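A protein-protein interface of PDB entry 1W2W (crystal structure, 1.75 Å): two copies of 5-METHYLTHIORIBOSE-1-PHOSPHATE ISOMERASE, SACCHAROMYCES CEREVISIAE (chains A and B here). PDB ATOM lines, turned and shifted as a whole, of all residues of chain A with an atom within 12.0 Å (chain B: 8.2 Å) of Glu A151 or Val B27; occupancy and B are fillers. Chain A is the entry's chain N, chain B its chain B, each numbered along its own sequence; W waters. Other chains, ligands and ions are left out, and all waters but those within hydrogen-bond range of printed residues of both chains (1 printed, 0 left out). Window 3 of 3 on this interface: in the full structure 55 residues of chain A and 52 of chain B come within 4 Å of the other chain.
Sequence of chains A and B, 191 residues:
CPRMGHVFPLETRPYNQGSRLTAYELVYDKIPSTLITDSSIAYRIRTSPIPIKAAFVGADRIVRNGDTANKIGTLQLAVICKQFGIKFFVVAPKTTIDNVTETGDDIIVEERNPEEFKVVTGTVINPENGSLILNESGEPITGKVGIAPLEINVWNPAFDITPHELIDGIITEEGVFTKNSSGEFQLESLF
No position is printed for both chains.
The backbone carbonyl oxygen of Ile A152 lies within hydrogen-bond range of the side-chain amino group of Lys A118 (2.8 Å). The backbone carbonyl oxygen (O) of Ile B31 lies within hydrogen-bond range of the side-chain hydroxyl (OG) of Ser B33 (2.7 Å). The side-chain amino group (NZ) of Lys A118 sits at hydrogen-bond distance from the backbone carbonyl oxygen (O) of Pro A149, 2.9 Å away. N of Ile A147 lies within hydrogen-bond range of O of Lys A118.
Water W1 bridges N of Asn A153 (2.8 Å) and O of Ser B33 (2.8 Å).
Glu A151 touches just one residue of chain B: Val B27 (3.7 Å). Of the printed residues of chain A, Val B27 touches Glu A151 and Ile A152. Of chain A, only Pro A149 and Ile A152 come within 4 Å of Ala B23. No residue of chain A comes within 4 Å of Leu B26. No residue of chain A comes within 4 Å of Asp B29. No residue of chain A comes within 4 Å of Lys B30. Of the printed residues of chain B, Ile A147 touches Ser B19. Of the printed residues of chain B, Ala A148 touches Ser B19. Of the printed residues of chain B, Asn A153 touches Ser B33 (3.5 Å). Printed residues of chain B within 4 Å of Ile A152: Ala B23, Val B27 and Ser B33. Of the printed residues of chain A, Tyr B24 touches Pro A149 (3.8 Å). Lys A118 touches none of the printed residues of chain B. The nearest residue of chain A that does not touch Val B27 is Pro A149 (4.5 Å).
Hydrophobic or aromatic side chains of chain B that line the printed part of chain A: Ala B23 and Val B27.
Ser B19 touches Ala A148. Ser B19 touches Pro A149. CD of Pro A149 touches CB of Ala B23 (3.9 Å). Tyr B24 touches Pro A149 (N to CG, 3.8 Å). Val B27 touches Glu A151 (CG1 to CB, 3.7 Å). CG1 of Ile A152 touches CB of Ala B23, at 3.8 Å. N of Ile A152 touches CG2 of Val B27, 3.8 Å away. Ser B33 touches Ile A152. Asn A153 touches Ser B33.
O of Ile A147 is in hydrogen-bond range of OG of Ser B19 (2.7 Å).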
ATOM      1  N   PRO A 114      23.045 -13.402  15.920  1.00  0.00           N
ATOM      2  CA  PRO A 114      22.431 -12.070  15.818  1.00  0.00           C
ATOM      3  C   PRO A 114      21.041 -12.068  15.170  1.00  0.00           C
ATOM      4  O   PRO A 114      20.222 -11.202  15.492  1.00  0.00           O
ATOM      5  CB  PRO A 114      23.425 -11.283  14.955  1.00  0.00           C
ATOM      6  CG  PRO A 114      24.252 -12.329  14.256  1.00  0.00           C
ATOM      7  CD  PRO A 114      24.344 -13.471  15.229  1.00  0.00           C
ATOM      8  N   GLU A 115      20.774 -13.018  14.277  1.00  0.00           N
ATOM      9  CA  GLU A 115      19.450 -13.098  13.668  1.00  0.00           C
ATOM     10  C   GLU A 115      18.332 -13.370  14.676  1.00  0.00           C
ATOM     11  O   GLU A 115      17.180 -13.027  14.425  1.00  0.00           O
ATOM     12  CB  GLU A 115      19.416 -14.103  12.510  1.00  0.00           C
ATOM     13  CG  GLU A 115      20.195 -13.643  11.284  1.00  0.00           C
ATOM     14  CD  GLU A 115      19.694 -12.326  10.700  1.00  0.00           C
ATOM     15  OE1 GLU A 115      18.843 -12.355   9.776  1.00  0.00           O
ATOM     16  OE2 GLU A 115      20.160 -11.257  11.156  1.00  0.00           O
ATOM     17  N   PHE A 117      18.006 -11.919  17.421  1.00  0.00           N
ATOM     18  CA  PHE A 117      17.746 -10.598  18.000  1.00  0.00           C
ATOM     19  C   PHE A 117      17.043  -9.765  16.915  1.00  0.00           C
ATOM     20  O   PHE A 117      16.026  -9.106  17.179  1.00  0.00           O
ATOM     21  CB  PHE A 117      19.110 -10.016  18.411  1.00  0.00           C
ATOM     22  CG  PHE A 117      19.086  -8.593  18.920  1.00  0.00           C
ATOM     23  CD1 PHE A 117      19.889  -8.231  19.991  1.00  0.00           C
ATOM     24  CD2 PHE A 117      18.295  -7.613  18.328  1.00  0.00           C
ATOM     25  CE1 PHE A 117      19.894  -6.929  20.483  1.00  0.00           C
ATOM     26  CE2 PHE A 117      18.298  -6.302  18.816  1.00  0.00           C
ATOM     27  CZ  PHE A 117      19.097  -5.965  19.894  1.00  0.00           C
ATOM     28  N   LYS A 118      17.562  -9.805  15.683  1.00  0.00           N
ATOM     29  CA  LYS A 118      17.097  -8.900  14.641  1.00  0.00           C
ATOM     30  C   LYS A 118      15.787  -9.329  14.015  1.00  0.00           C
ATOM     31  O   LYS A 118      15.107  -8.526  13.376  1.00  0.00           O
ATOM     32  CB  LYS A 118      18.123  -8.833  13.523  1.00  0.00           C
ATOM     33  CG  LYS A 118      19.374  -8.099  13.909  1.00  0.00           C
ATOM     34  CD  LYS A 118      20.163  -7.929  12.639  1.00  0.00           C
ATOM     35  CE  LYS A 118      21.497  -7.307  12.886  1.00  0.00           C
ATOM     36  NZ  LYS A 118      22.056  -7.013  11.537  1.00  0.00           N
ATOM     37  N   VAL A 119      15.457 -10.603  14.182  1.00  0.00           N
ATOM     38  CA  VAL A 119      14.244 -11.159  13.588  1.00  0.00           C
ATOM     39  C   VAL A 119      13.332 -11.655  14.698  1.00  0.00           C
ATOM     40  O   VAL A 119      13.788 -12.353  15.600  1.00  0.00           O
ATOM     41  CB  VAL A 119      14.592 -12.324  12.640  1.00  0.00           C
ATOM     42  CG1 VAL A 119      13.312 -13.027  12.165  1.00  0.00           C
ATOM     43  CG2 VAL A 119      15.397 -11.799  11.463  1.00  0.00           C
ATOM     44  N   GLY A 146      11.698  -8.859  10.327  1.00  0.00           N
ATOM     45  CA  GLY A 146      12.961  -8.217  10.661  1.00  0.00           C
ATOM     46  C   GLY A 146      12.783  -6.804  11.192  1.00  0.00           C
ATOM     47  O   GLY A 146      12.033  -6.013  10.625  1.00  0.00           O
ATOM     48  N   ILE A 147      13.468  -6.499  12.293  1.00  0.00           N
ATOM     49  CA  ILE A 147      13.279  -5.228  12.984  1.00  0.00           C
ATOM     50  C   ILE A 147      14.554  -4.388  13.068  1.00  0.00           C
ATOM     51  O   ILE A 147      14.617  -3.406  13.813  1.00  0.00           O
ATOM     52  CB  ILE A 147      12.593  -5.401  14.371  1.00  0.00           C
ATOM     53  CG1 ILE A 147      13.359  -6.351  15.294  1.00  0.00           C
ATOM     54  CG2 ILE A 147      11.159  -5.910  14.199  1.00  0.00           C
ATOM     55  CD1 ILE A 147      14.733  -5.860  15.713  1.00  0.00           C
ATOM     56  N   ALA A 148      15.568  -4.771  12.298  1.00  0.00           N
ATOM     57  CA  ALA A 148      16.799  -3.987  12.276  1.00  0.00           C
ATOM     58  C   ALA A 148      17.491  -4.178  10.935  1.00  0.00           C
ATOM     59  O   ALA A 148      17.281  -5.199  10.268  1.00  0.00           O
ATOM     60  CB  ALA A 148      17.714  -4.441  13.435  1.00  0.00           C
ATOM     61  N   PRO A 149      18.322  -3.217  10.539  1.00  0.00           N
ATOM     62  CA  PRO A 149      19.084  -3.350   9.291  1.00  0.00           C
ATOM     63  C   PRO A 149      19.986  -4.571   9.319  1.00  0.00           C
ATOM     64  O   PRO A 149      20.533  -4.897  10.370  1.00  0.00           O
ATOM     65  CB  PRO A 149      19.958  -2.090   9.257  1.00  0.00           C
ATOM     66  CG  PRO A 149      19.321  -1.121  10.206  1.00  0.00           C
ATOM     67  CD  PRO A 149      18.596  -1.948  11.245  1.00  0.00           C
ATOM     68  N   LEU A 150      20.125  -5.215   8.166  1.00  0.00           N
ATOM     69  CA  LEU A 150      21.159  -6.226   7.942  1.00  0.00           C
ATOM     70  C   LEU A 150      22.527  -5.777   8.474  1.00  0.00           C
ATOM     71  O   LEU A 150      23.234  -6.569   9.095  1.00  0.00           O
ATOM     72  CB  LEU A 150      21.233  -6.548   6.446  1.00  0.00           C
ATOM     73  CG  LEU A 150      22.264  -7.551   5.907  1.00  0.00           C
ATOM     74  CD1 LEU A 150      21.982  -8.967   6.398  1.00  0.00           C
ATOM     75  CD2 LEU A 150      22.259  -7.502   4.383  1.00  0.00           C
ATOM     76  N   GLU A 151      22.878  -4.509   8.240  1.00  0.00           N
ATOM     77  CA  GLU A 151      24.239  -4.002   8.463  1.00  0.00           C
ATOM     78  C   GLU A 151      24.627  -3.772   9.933  1.00  0.00           C
ATOM     79  O   GLU A 151      25.814  -3.819  10.279  1.00  0.00           O
ATOM     80  CB  GLU A 151      24.490  -2.716   7.670  1.00  0.00           C
ATOM     81  CG  GLU A 151      24.458  -2.878   6.162  1.00  0.00           C
ATOM     82  CD  GLU A 151      23.075  -2.643   5.575  1.00  0.00           C
ATOM     83  OE1 GLU A 151      22.076  -2.628   6.335  1.00  0.00           O
ATOM     84  OE2 GLU A 151      22.994  -2.482   4.342  1.00  0.00           O
ATOM     85  N   ILE A 152      23.655  -3.526  10.798  1.00  0.00           N
ATOM     86  CA  ILE A 152      23.964  -3.269  12.212  1.00  0.00           C
ATOM     87  C   ILE A 152      24.529  -4.484  12.974  1.00  0.00           C
ATOM     88  O   ILE A 152      23.981  -5.594  12.952  1.00  0.00           O
ATOM     89  CB  ILE A 152      22.776  -2.584  12.943  1.00  0.00           C
ATOM     90  CG1 ILE A 152      23.234  -1.864  14.224  1.00  0.00           C
ATOM     91  CG2 ILE A 152      21.667  -3.582  13.272  1.00  0.00           C
ATOM     92  CD1 ILE A 152      23.827  -0.481  13.985  1.00  0.00           C
ATOM     93  N   ASN A 153      25.650  -4.265  13.653  1.00  0.00           N
ATOM     94  CA  ASN A 153      26.157  -5.209  14.651  1.00  0.00           C
ATOM     95  C   ASN A 153      25.224  -5.231  15.864  1.00  0.00           C
ATOM     96  O   ASN A 153      24.718  -4.190  16.268  1.00  0.00           O
ATOM     97  CB  ASN A 153      27.557  -4.744  15.068  1.00  0.00           C
ATOM     98  CG  ASN A 153      28.289  -5.745  15.925  1.00  0.00           C
ATOM     99  OD1 ASN A 153      28.798  -5.403  16.997  1.00  0.00           O
ATOM    100  ND2 ASN A 153      28.364  -6.983  15.462  1.00  0.00           N
ATOM    101  N   VAL A 154      24.980  -6.407  16.437  1.00  0.00           N
ATOM    102  CA  VAL A 154      24.230  -6.512  17.682  1.00  0.00           C
ATOM    103  C   VAL A 154      25.003  -7.294  18.739  1.00  0.00           C
ATOM    104  O   VAL A 154      25.911  -8.066  18.431  1.00  0.00           O
ATOM    105  CB  VAL A 154      22.849  -7.173  17.484  1.00  0.00           C
ATOM    106  CG1 VAL A 154      21.992  -6.368  16.507  1.00  0.00           C
ATOM    107  CG2 VAL A 154      23.016  -8.618  17.026  1.00  0.00           C
ATOM    108  N   TRP A 155      24.636  -7.082  19.996  1.00  0.00           N
ATOM    109  CA  TRP A 155      25.158  -7.863  21.109  1.00  0.00           C
ATOM    110  C   TRP A 155      24.010  -8.712  21.598  1.00  0.00           C
ATOM    111  O   TRP A 155      22.947  -8.190  21.934  1.00  0.00           O
ATOM    112  CB  TRP A 155      25.618  -6.921  22.226  1.00  0.00           C
ATOM    113  CG  TRP A 155      26.411  -7.552  23.343  1.00  0.00           C
ATOM    114  CD1 TRP A 155      27.434  -8.455  23.241  1.00  0.00           C
ATOM    115  CD2 TRP A 155      26.232  -7.308  24.741  1.00  0.00           C
ATOM    116  NE1 TRP A 155      27.896  -8.786  24.493  1.00  0.00           N
ATOM    117  CE2 TRP A 155      27.174  -8.092  25.432  1.00  0.00           C
ATOM    118  CE3 TRP A 155      25.365  -6.498  25.481  1.00  0.00           C
ATOM    119  CZ2 TRP A 155      27.271  -8.096  26.822  1.00  0.00           C
ATOM    120  CZ3 TRP A 155      25.459  -6.497  26.863  1.00  0.00           C
ATOM    121  CH2 TRP A 155      26.409  -7.290  27.523  1.00  0.00           C
ATOM    122  N   SER B  19      16.007   0.132  17.025  1.00  0.00           N
ATOM    123  CA  SER B  19      16.478  -0.925  16.144  1.00  0.00           C
ATOM    124  C   SER B  19      16.132  -0.610  14.684  1.00  0.00           C
ATOM    125  O   SER B  19      16.883  -0.944  13.757  1.00  0.00           O
ATOM    126  CB  SER B  19      15.912  -2.283  16.585  1.00  0.00           C
ATOM    127  OG  SER B  19      14.517  -2.367  16.331  1.00  0.00           O
ATOM    128  N   LEU B  21      15.199   2.634  13.399  1.00  0.00           N
ATOM    129  CA  LEU B  21      15.468   3.989  12.905  1.00  0.00           C
ATOM    130  C   LEU B  21      16.888   4.444  13.262  1.00  0.00           C
ATOM    131  O   LEU B  21      17.672   4.820  12.380  1.00  0.00           O
ATOM    132  CB  LEU B  21      14.399   4.980  13.403  1.00  0.00           C
ATOM    133  CG  LEU B  21      12.929   4.594  13.180  1.00  0.00           C
ATOM    134  CD1 LEU B  21      11.991   5.654  13.810  1.00  0.00           C
ATOM    135  CD2 LEU B  21      12.606   4.409  11.692  1.00  0.00           C
ATOM    136  N   THR B  22      17.233   4.407  14.541  1.00  0.00           N
ATOM    137  CA  THR B  22      18.570   4.850  14.953  1.00  0.00           C
ATOM    138  C   THR B  22      19.674   3.948  14.367  1.00  0.00           C
ATOM    139  O   THR B  22      20.700   4.428  13.873  1.00  0.00           O
ATOM    140  CB  THR B  22      18.635   4.904  16.478  1.00  0.00           C
ATOM    141  OG1 THR B  22      17.842   6.005  16.936  1.00  0.00           O
ATOM    142  CG2 THR B  22      20.064   5.206  16.969  1.00  0.00           C
ATOM    143  N   ALA B  23      19.462   2.640  14.408  1.00  0.00           N
ATOM    144  CA  ALA B  23      20.448   1.735  13.818  1.00  0.00           C
ATOM    145  C   ALA B  23      20.620   2.015  12.310  1.00  0.00           C
ATOM    146  O   ALA B  23      21.724   1.942  11.777  1.00  0.00           O
ATOM    147  CB  ALA B  23      20.058   0.270  14.074  1.00  0.00           C
ATOM    148  N   TYR B  24      19.526   2.349  11.634  1.00  0.00           N
ATOM    149  CA  TYR B  24      19.570   2.770  10.236  1.00  0.00           C
ATOM    150  C   TYR B  24      20.428   4.021  10.030  1.00  0.00           C
ATOM    151  O   TYR B  24      21.276   4.069   9.123  1.00  0.00           O
ATOM    152  CB  TYR B  24      18.140   3.054   9.785  1.00  0.00           C
ATOM    153  CG  TYR B  24      17.935   3.292   8.309  1.00  0.00           C
ATOM    154  CD1 TYR B  24      18.501   2.456   7.360  1.00  0.00           C
ATOM    155  CD2 TYR B  24      17.154   4.358   7.869  1.00  0.00           C
ATOM    156  CE1 TYR B  24      18.299   2.672   6.003  1.00  0.00           C
ATOM    157  CE2 TYR B  24      16.950   4.586   6.518  1.00  0.00           C
ATOM    158  CZ  TYR B  24      17.525   3.736   5.596  1.00  0.00           C
ATOM    159  OH  TYR B  24      17.322   3.954   4.254  1.00  0.00           O
ATOM    160  N   GLU B  25      20.204   5.042  10.852  1.00  0.00           N
ATOM    161  CA  GLU B  25      20.988   6.267  10.734  1.00  0.00           C
ATOM    162  C   GLU B  25      22.475   6.007  10.984  1.00  0.00           C
ATOM    163  O   GLU B  25      23.334   6.549  10.282  1.00  0.00           O
ATOM    164  CB  GLU B  25      20.458   7.358  11.669  1.00  0.00           C
ATOM    165  CG  GLU B  25      19.031   7.793  11.346  1.00  0.00           C
ATOM    166  CD  GLU B  25      18.715   9.204  11.802  1.00  0.00           C
ATOM    167  OE1 GLU B  25      19.524  10.134  11.516  1.00  0.00           O
ATOM    168  OE2 GLU B  25      17.660   9.391  12.447  1.00  0.00           O
ATOM    169  N   LEU B  26      22.784   5.176  11.982  1.00  0.00           N
ATOM    170  CA  LEU B  26      24.176   4.928  12.350  1.00  0.00           C
ATOM    171  C   LEU B  26      24.889   4.168  11.231  1.00  0.00           C
ATOM    172  O   LEU B  26      26.056   4.437  10.915  1.00  0.00           O
ATOM    173  CB  LEU B  26      24.255   4.140  13.671  1.00  0.00           C
ATOM    174  CG  LEU B  26      23.846   4.968  14.896  1.00  0.00           C
ATOM    175  CD1 LEU B  26      23.572   4.070  16.124  1.00  0.00           C
ATOM    176  CD2 LEU B  26      24.919   5.999  15.197  1.00  0.00           C
ATOM    177  N   VAL B  27      24.170   3.233  10.619  1.00  0.00           N
ATOM    178  CA  VAL B  27      24.680   2.486   9.468  1.00  0.00           C
ATOM    179  C   VAL B  27      24.967   3.419   8.304  1.00  0.00           C
ATOM    180  O   VAL B  27      26.051   3.392   7.706  1.00  0.00           O
ATOM    181  CB  VAL B  27      23.674   1.390   9.028  1.00  0.00           C
ATOM    182  CG1 VAL B  27      23.919   0.961   7.579  1.00  0.00           C
ATOM    183  CG2 VAL B  27      23.765   0.197   9.971  1.00  0.00           C
ATOM    184  N   TYR B  28      23.986   4.255   7.989  1.00  0.00           N
ATOM    185  CA  TYR B  28      24.145   5.258   6.940  1.00  0.00           C
ATOM    186  C   TYR B  28      25.386   6.135   7.128  1.00  0.00           C
ATOM    187  O   TYR B  28      26.110   6.440   6.157  1.00  0.00           O
ATOM    188  CB  TYR B  28      22.883   6.110   6.882  1.00  0.00           C
ATOM    189  CG  TYR B  28      22.882   7.182   5.818  1.00  0.00           C
ATOM    190  CD1 TYR B  28      22.377   6.921   4.552  1.00  0.00           C
ATOM    191  CD2 TYR B  28      23.367   8.456   6.088  1.00  0.00           C
ATOM    192  CE1 TYR B  28      22.359   7.905   3.575  1.00  0.00           C
ATOM    193  CE2 TYR B  28      23.356   9.447   5.115  1.00  0.00           C
ATOM    194  CZ  TYR B  28      22.850   9.160   3.862  1.00  0.00           C
ATOM    195  OH  TYR B  28      22.832  10.137   2.885  1.00  0.00           O
ATOM    196  N   ASP B  29      25.636   6.540   8.370  1.00  0.00           N
ATOM    197  CA  ASP B  29      26.709   7.487   8.664  1.00  0.00           C
ATOM    198  C   ASP B  29      28.041   6.798   8.934  1.00  0.00           C
ATOM    199  O   ASP B  29      29.052   7.475   9.160  1.00  0.00           O
ATOM    200  CB  ASP B  29      26.358   8.361   9.870  1.00  0.00           C
ATOM    201  CG  ASP B  29      25.371   9.454   9.531  1.00  0.00           C
ATOM    202  OD1 ASP B  29      25.295   9.867   8.352  1.00  0.00           O
ATOM    203  OD2 ASP B  29      24.635   9.969  10.387  1.00  0.00           O
ATOM    204  N   LYS B  30      28.022   5.465   8.917  1.00  0.00           N
ATOM    205  CA  LYS B  30      29.206   4.646   9.153  1.00  0.00           C
ATOM    206  C   LYS B  30      29.816   4.924  10.527  1.00  0.00           C
ATOM    207  O   LYS B  30      31.037   4.967  10.699  1.00  0.00           O
ATOM    208  CB  LYS B  30      30.216   4.818   8.005  1.00  0.00           C
ATOM    209  CG  LYS B  30      29.555   4.593   6.645  1.00  0.00           C
ATOM    210  CD  LYS B  30      30.529   4.635   5.475  1.00  0.00           C
ATOM    211  CE  LYS B  30      29.765   4.684   4.157  1.00  0.00           C
ATOM    212  NZ  LYS B  30      30.602   4.185   3.031  1.00  0.00           N
ATOM    213  N   ILE B  31      28.955   5.097  11.526  1.00  0.00           N
ATOM    214  CA  ILE B  31      29.446   5.297  12.885  1.00  0.00           C
ATOM    215  C   ILE B  31      29.465   3.934  13.578  1.00  0.00           C
ATOM    216  O   ILE B  31      28.444   3.249  13.607  1.00  0.00           O
ATOM    217  CB  ILE B  31      28.525   6.289  13.641  1.00  0.00           C
ATOM    218  CG1 ILE B  31      28.512   7.643  12.931  1.00  0.00           C
ATOM    219  CG2 ILE B  31      28.971   6.432  15.111  1.00  0.00           C
ATOM    220  CD1 ILE B  31      27.502   8.633  13.506  1.00  0.00           C
ATOM    221  N   PRO B  32      30.613   3.532  14.122  1.00  0.00           N
ATOM    222  CA  PRO B  32      30.741   2.209  14.750  1.00  0.00           C
ATOM    223  C   PRO B  32      29.769   2.035  15.917  1.00  0.00           C
ATOM    224  O   PRO B  32      29.816   2.792  16.888  1.00  0.00           O
ATOM    225  CB  PRO B  32      32.171   2.209  15.297  1.00  0.00           C
ATOM    226  CG  PRO B  32      32.898   3.199  14.411  1.00  0.00           C
ATOM    227  CD  PRO B  32      31.877   4.289  14.150  1.00  0.00           C
ATOM    228  N   SER B  33      28.905   1.031  15.810  1.00  0.00           N
ATOM    229  CA  SER B  33      27.749   0.921  16.690  1.00  0.00           C
ATOM    230  C   SER B  33      27.420  -0.544  16.929  1.00  0.00           C
ATOM    231  O   SER B  33      27.652  -1.388  16.066  1.00  0.00           O
ATOM    232  CB  SER B  33      26.542   1.539  15.991  1.00  0.00           C
ATOM    233  OG  SER B  33      26.771   2.912  15.755  1.00  0.00           O
HETATM  234  O   HOH W   1      27.044  -1.826  13.338  1.00  0.00           O
